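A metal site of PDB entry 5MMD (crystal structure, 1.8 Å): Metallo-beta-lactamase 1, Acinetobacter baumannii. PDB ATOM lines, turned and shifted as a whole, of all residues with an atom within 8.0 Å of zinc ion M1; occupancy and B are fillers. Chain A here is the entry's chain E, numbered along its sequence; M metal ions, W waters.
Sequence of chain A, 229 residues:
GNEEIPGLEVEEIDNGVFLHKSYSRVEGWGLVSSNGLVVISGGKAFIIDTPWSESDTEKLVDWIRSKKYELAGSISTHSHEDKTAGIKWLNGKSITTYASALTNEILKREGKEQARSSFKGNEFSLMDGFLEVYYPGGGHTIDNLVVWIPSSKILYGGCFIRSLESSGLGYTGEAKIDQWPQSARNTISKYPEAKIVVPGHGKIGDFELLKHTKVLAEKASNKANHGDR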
ATOM      1  N   THR A  77     -23.827   5.199   3.738  1.00  0.00           N
ATOM      2  CA  THR A  77     -23.593   5.019   5.169  1.00  0.00           C
ATOM      3  C   THR A  77     -22.182   4.541   5.504  1.00  0.00           C
ATOM      4  O   THR A  77     -21.801   4.504   6.667  1.00  0.00           O
ATOM      5  CB  THR A  77     -24.651   4.038   5.781  1.00  0.00           C
ATOM      6  OG1 THR A  77     -24.533   2.742   5.172  1.00  0.00           O
ATOM      7  CG2 THR A  77     -26.033   4.566   5.542  1.00  0.00           C
ATOM      8  N   HIS A  78     -21.410   4.150   4.481  1.00  0.00           N
ATOM      9  CA  HIS A  78     -19.940   4.186   4.633  1.00  0.00           C
ATOM     10  C   HIS A  78     -19.344   4.163   3.237  1.00  0.00           C
ATOM     11  O   HIS A  78     -20.092   4.128   2.247  1.00  0.00           O
ATOM     12  CB  HIS A  78     -19.399   3.040   5.508  1.00  0.00           C
ATOM     13  CG  HIS A  78     -19.622   1.654   4.982  1.00  0.00           C
ATOM     14  ND1 HIS A  78     -20.856   1.041   4.964  1.00  0.00           N
ATOM     15  CD2 HIS A  78     -18.732   0.711   4.548  1.00  0.00           C
ATOM     16  CE1 HIS A  78     -20.729  -0.186   4.488  1.00  0.00           C
ATOM     17  NE2 HIS A  78     -19.446  -0.411   4.249  1.00  0.00           N
ATOM     18  N   SER A  79     -18.014   4.140   3.146  1.00  0.00           N
ATOM     19  CA  SER A  79     -17.353   4.361   1.871  1.00  0.00           C
ATOM     20  C   SER A  79     -17.367   3.185   0.872  1.00  0.00           C
ATOM     21  O   SER A  79     -17.187   3.408  -0.323  1.00  0.00           O
ATOM     22  CB  SER A  79     -15.879   4.767   2.113  1.00  0.00           C
ATOM     23  OG  SER A  79     -15.148   3.686   2.638  1.00  0.00           O
ATOM     24  N   HIS A  80     -17.601   1.951   1.348  1.00  0.00           N
ATOM     25  CA  HIS A  80     -17.471   0.763   0.477  1.00  0.00           C
ATOM     26  C   HIS A  80     -18.384   0.809  -0.750  1.00  0.00           C
ATOM     27  O   HIS A  80     -19.481   1.398  -0.739  1.00  0.00           O
ATOM     28  CB  HIS A  80     -17.684  -0.528   1.258  1.00  0.00           C
ATOM     29  CG  HIS A  80     -16.566  -0.844   2.202  1.00  0.00           C
ATOM     30  ND1 HIS A  80     -16.705  -1.702   3.267  1.00  0.00           N
ATOM     31  CD2 HIS A  80     -15.271  -0.423   2.209  1.00  0.00           C
ATOM     32  CE1 HIS A  80     -15.546  -1.808   3.899  1.00  0.00           C
ATOM     33  NE2 HIS A  80     -14.663  -1.027   3.284  1.00  0.00           N
ATOM     34  N   GLU A  81     -17.871   0.238  -1.820  1.00  0.00           N
ATOM     35  CA  GLU A  81     -18.507   0.263  -3.127  1.00  0.00           C
ATOM     36  C   GLU A  81     -19.952  -0.259  -3.126  1.00  0.00           C
ATOM     37  O   GLU A  81     -20.755   0.183  -3.947  1.00  0.00           O
ATOM     38  CB  GLU A  81     -17.679  -0.543  -4.103  1.00  0.00           C
ATOM     39  CG  GLU A  81     -18.052  -0.403  -5.558  1.00  0.00           C
ATOM     40  CD  GLU A  81     -17.727   0.943  -6.164  1.00  0.00           C
ATOM     41  OE1 GLU A  81     -18.072   1.108  -7.343  1.00  0.00           O
ATOM     42  OE2 GLU A  81     -17.102   1.816  -5.521  1.00  0.00           O
ATOM     43  N   ASP A  82     -20.284  -1.165  -2.211  1.00  0.00           N
ATOM     44  CA  ASP A  82     -21.649  -1.702  -2.195  1.00  0.00           C
ATOM     45  C   ASP A  82     -22.677  -0.616  -1.807  1.00  0.00           C
ATOM     46  O   ASP A  82     -23.841  -0.793  -2.084  1.00  0.00           O
ATOM     47  CB  ASP A  82     -21.802  -2.971  -1.297  1.00  0.00           C
ATOM     48  CG  ASP A  82     -21.320  -2.795   0.130  1.00  0.00           C
ATOM     49  OD1 ASP A  82     -20.342  -2.040   0.326  1.00  0.00           O
ATOM     50  OD2 ASP A  82     -21.859  -3.512   1.048  1.00  0.00           O
ATOM     51  N   LYS A  83     -22.256   0.490  -1.216  1.00  0.00           N
ATOM     52  CA  LYS A  83     -23.193   1.542  -0.757  1.00  0.00           C
ATOM     53  C   LYS A  83     -22.985   2.897  -1.445  1.00  0.00           C
ATOM     54  O   LYS A  83     -23.822   3.825  -1.289  1.00  0.00           O
ATOM     55  CB  LYS A  83     -23.046   1.723   0.757  1.00  0.00           C
ATOM     56  CG  LYS A  83     -23.182   0.481   1.595  1.00  0.00           C
ATOM     57  CD  LYS A  83     -24.455  -0.340   1.314  1.00  0.00           C
ATOM     58  CE  LYS A  83     -24.513  -1.561   2.245  1.00  0.00           C
ATOM     59  NZ  LYS A  83     -25.580  -2.465   1.845  1.00  0.00           N
ATOM     60  N   HIS A 140     -17.899  -2.323  11.577  1.00  0.00           N
ATOM     61  CA  HIS A 140     -17.595  -2.784  10.230  1.00  0.00           C
ATOM     62  C   HIS A 140     -16.466  -1.952   9.613  1.00  0.00           C
ATOM     63  O   HIS A 140     -15.584  -2.505   8.956  1.00  0.00           O
ATOM     64  CB  HIS A 140     -18.842  -2.712   9.402  1.00  0.00           C
ATOM     65  CG  HIS A 140     -18.626  -2.973   7.948  1.00  0.00           C
ATOM     66  ND1 HIS A 140     -18.298  -4.220   7.456  1.00  0.00           N
ATOM     67  CD2 HIS A 140     -18.679  -2.140   6.880  1.00  0.00           C
ATOM     68  CE1 HIS A 140     -18.161  -4.129   6.134  1.00  0.00           C
ATOM     69  NE2 HIS A 140     -18.387  -2.880   5.758  1.00  0.00           N
ATOM     70  N   THR A 141     -16.575  -0.618   9.785  1.00  0.00           N
ATOM     71  CA  THR A 141     -15.573   0.336   9.342  1.00  0.00           C
ATOM     72  C   THR A 141     -15.537   1.500  10.325  1.00  0.00           C
ATOM     73  O   THR A 141     -16.429   1.675  11.179  1.00  0.00           O
ATOM     74  CB  THR A 141     -15.842   0.876   7.903  1.00  0.00           C
ATOM     75  OG1 THR A 141     -17.152   1.483   7.829  1.00  0.00           O
ATOM     76  CG2 THR A 141     -15.708  -0.245   6.868  1.00  0.00           C
ATOM     77  N   ASP A 143     -16.091   4.501   9.599  1.00  0.00           N
ATOM     78  CA  ASP A 143     -17.041   5.587   9.254  1.00  0.00           C
ATOM     79  C   ASP A 143     -18.507   5.159   9.285  1.00  0.00           C
ATOM     80  O   ASP A 143     -19.380   5.995   9.021  1.00  0.00           O
ATOM     81  CB  ASP A 143     -16.719   6.165   7.878  1.00  0.00           C
ATOM     82  CG  ASP A 143     -16.750   5.114   6.758  1.00  0.00           C
ATOM     83  OD1 ASP A 143     -16.434   3.951   7.031  1.00  0.00           O
ATOM     84  OD2 ASP A 143     -17.059   5.455   5.582  1.00  0.00           O
ATOM     85  N   ASN A 144     -18.784   3.900   9.620  1.00  0.00           N
ATOM     86  CA  ASN A 144     -20.141   3.367   9.369  1.00  0.00           C
ATOM     87  C   ASN A 144     -21.188   4.167  10.165  1.00  0.00           C
ATOM     88  O   ASN A 144     -20.999   4.500  11.337  1.00  0.00           O
ATOM     89  CB  ASN A 144     -20.294   1.849   9.631  1.00  0.00           C
ATOM     90  CG  ASN A 144     -19.686   1.346  10.937  1.00  0.00           C
ATOM     91  OD1 ASN A 144     -19.297   0.161  10.989  1.00  0.00           O
ATOM     92  ND2 ASN A 144     -19.659   2.147  11.986  1.00  0.00           N
ATOM     93  N   GLY A 158     -27.123  -0.792   8.090  1.00  0.00           N
ATOM     94  CA  GLY A 158     -26.035  -0.956   7.164  1.00  0.00           C
ATOM     95  C   GLY A 158     -25.095  -2.075   7.607  1.00  0.00           C
ATOM     96  O   GLY A 158     -25.461  -2.953   8.388  1.00  0.00           O
ATOM     97  N   CYS A 159     -23.881  -2.051   7.091  1.00  0.00           N
ATOM     98  CA  CYS A 159     -23.031  -3.217   7.295  1.00  0.00           C
ATOM     99  C   CYS A 159     -22.458  -3.242   8.684  1.00  0.00           C
ATOM    100  O   CYS A 159     -21.802  -4.194   9.048  1.00  0.00           O
ATOM    101  CB  CYS A 159     -21.954  -3.243   6.240  1.00  0.00           C
ATOM    102  SG  CYS A 159     -22.715  -3.157   4.635  1.00  0.00           S
ATOM    103  N   PHE A 160     -22.766  -2.207   9.468  1.00  0.00           N
ATOM    104  CA  PHE A 160     -22.486  -2.175  10.894  1.00  0.00           C
ATOM    105  C   PHE A 160     -23.288  -3.227  11.648  1.00  0.00           C
ATOM    106  O   PHE A 160     -22.944  -3.603  12.782  1.00  0.00           O
ATOM    107  CB  PHE A 160     -22.835  -0.779  11.455  1.00  0.00           C
ATOM    108  CG  PHE A 160     -22.676  -0.654  12.948  1.00  0.00           C
ATOM    109  CD1 PHE A 160     -21.417  -0.618  13.514  1.00  0.00           C
ATOM    110  CD2 PHE A 160     -23.793  -0.541  13.788  1.00  0.00           C
ATOM    111  CE1 PHE A 160     -21.251  -0.497  14.882  1.00  0.00           C
ATOM    112  CE2 PHE A 160     -23.629  -0.411  15.157  1.00  0.00           C
ATOM    113  CZ  PHE A 160     -22.345  -0.397  15.706  1.00  0.00           C
ATOM    114  N   TYR A 171     -16.870  -9.257   6.230  1.00  0.00           N
ATOM    115  CA  TYR A 171     -15.581  -8.698   5.808  1.00  0.00           C
ATOM    116  C   TYR A 171     -15.002  -7.774   6.868  1.00  0.00           C
ATOM    117  O   TYR A 171     -15.549  -6.704   7.142  1.00  0.00           O
ATOM    118  CB  TYR A 171     -15.719  -7.932   4.498  1.00  0.00           C
ATOM    119  CG  TYR A 171     -14.443  -7.180   4.141  1.00  0.00           C
ATOM    120  CD1 TYR A 171     -13.260  -7.862   3.865  1.00  0.00           C
ATOM    121  CD2 TYR A 171     -14.406  -5.780   4.114  1.00  0.00           C
ATOM    122  CE1 TYR A 171     -12.090  -7.171   3.526  1.00  0.00           C
ATOM    123  CE2 TYR A 171     -13.237  -5.081   3.787  1.00  0.00           C
ATOM    124  CZ  TYR A 171     -12.090  -5.784   3.514  1.00  0.00           C
ATOM    125  OH  TYR A 171     -10.924  -5.116   3.182  1.00  0.00           O
ATOM    126  N   GLU A 174     -11.204  -3.963   7.100  1.00  0.00           N
ATOM    127  CA  GLU A 174     -11.117  -2.548   7.520  1.00  0.00           C
ATOM    128  C   GLU A 174     -11.991  -2.259   8.769  1.00  0.00           C
ATOM    129  O   GLU A 174     -12.403  -1.135   8.988  1.00  0.00           O
ATOM    130  CB  GLU A 174     -11.522  -1.607   6.374  1.00  0.00           C
ATOM    131  CG  GLU A 174     -10.693  -1.776   5.101  1.00  0.00           C
ATOM    132  CD  GLU A 174     -11.495  -1.464   3.837  1.00  0.00           C
ATOM    133  OE1 GLU A 174     -12.037  -0.350   3.737  1.00  0.00           O
ATOM    134  OE2 GLU A 174     -11.579  -2.332   2.940  1.00  0.00           O
ATOM    135  N   HIS A 201     -26.349  -6.470   4.630  1.00  0.00           N
ATOM    136  CA  HIS A 201     -26.317  -7.739   3.886  1.00  0.00           C
ATOM    137  C   HIS A 201     -27.213  -8.733   4.603  1.00  0.00           C
ATOM    138  O   HIS A 201     -27.101  -8.934   5.835  1.00  0.00           O
ATOM    139  CB  HIS A 201     -24.882  -8.270   3.788  1.00  0.00           C
ATOM    140  CG  HIS A 201     -23.944  -7.343   3.094  1.00  0.00           C
ATOM    141  ND1 HIS A 201     -23.963  -7.164   1.720  1.00  0.00           N
ATOM    142  CD2 HIS A 201     -23.002  -6.485   3.569  1.00  0.00           C
ATOM    143  CE1 HIS A 201     -23.042  -6.283   1.381  1.00  0.00           C
ATOM    144  NE2 HIS A 201     -22.436  -5.865   2.488  1.00  0.00           N
HETATM  145 ZN    ZN M   1     -18.514  -2.311   3.931  1.00  0.00          ZN
HETATM  146 ZN    ZN M   2     -21.349  -4.017   2.914  1.00  0.00          ZN
HETATM  147  O   HOH W   1     -19.353  -3.482   2.844  1.00  0.00           O
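N of His 140 is in hydrogen-bond range of OD1 of Asn 144 (2.9 Å).
NE2 of His 80 sits at hydrogen-bond distance from OE1 of Glu 174 (2.7 Å).
Three residues have an atom within 4 Å of zinc ion M1: His 78, His 80 and His 140.
The nearest printed residue that does not touch zinc ion M1 is Asp 82 (4.1 Å).
Zinc ion M1 is bound by water W1, NE2 of His 140, ND1 of His 80 and NE2 of His 78.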
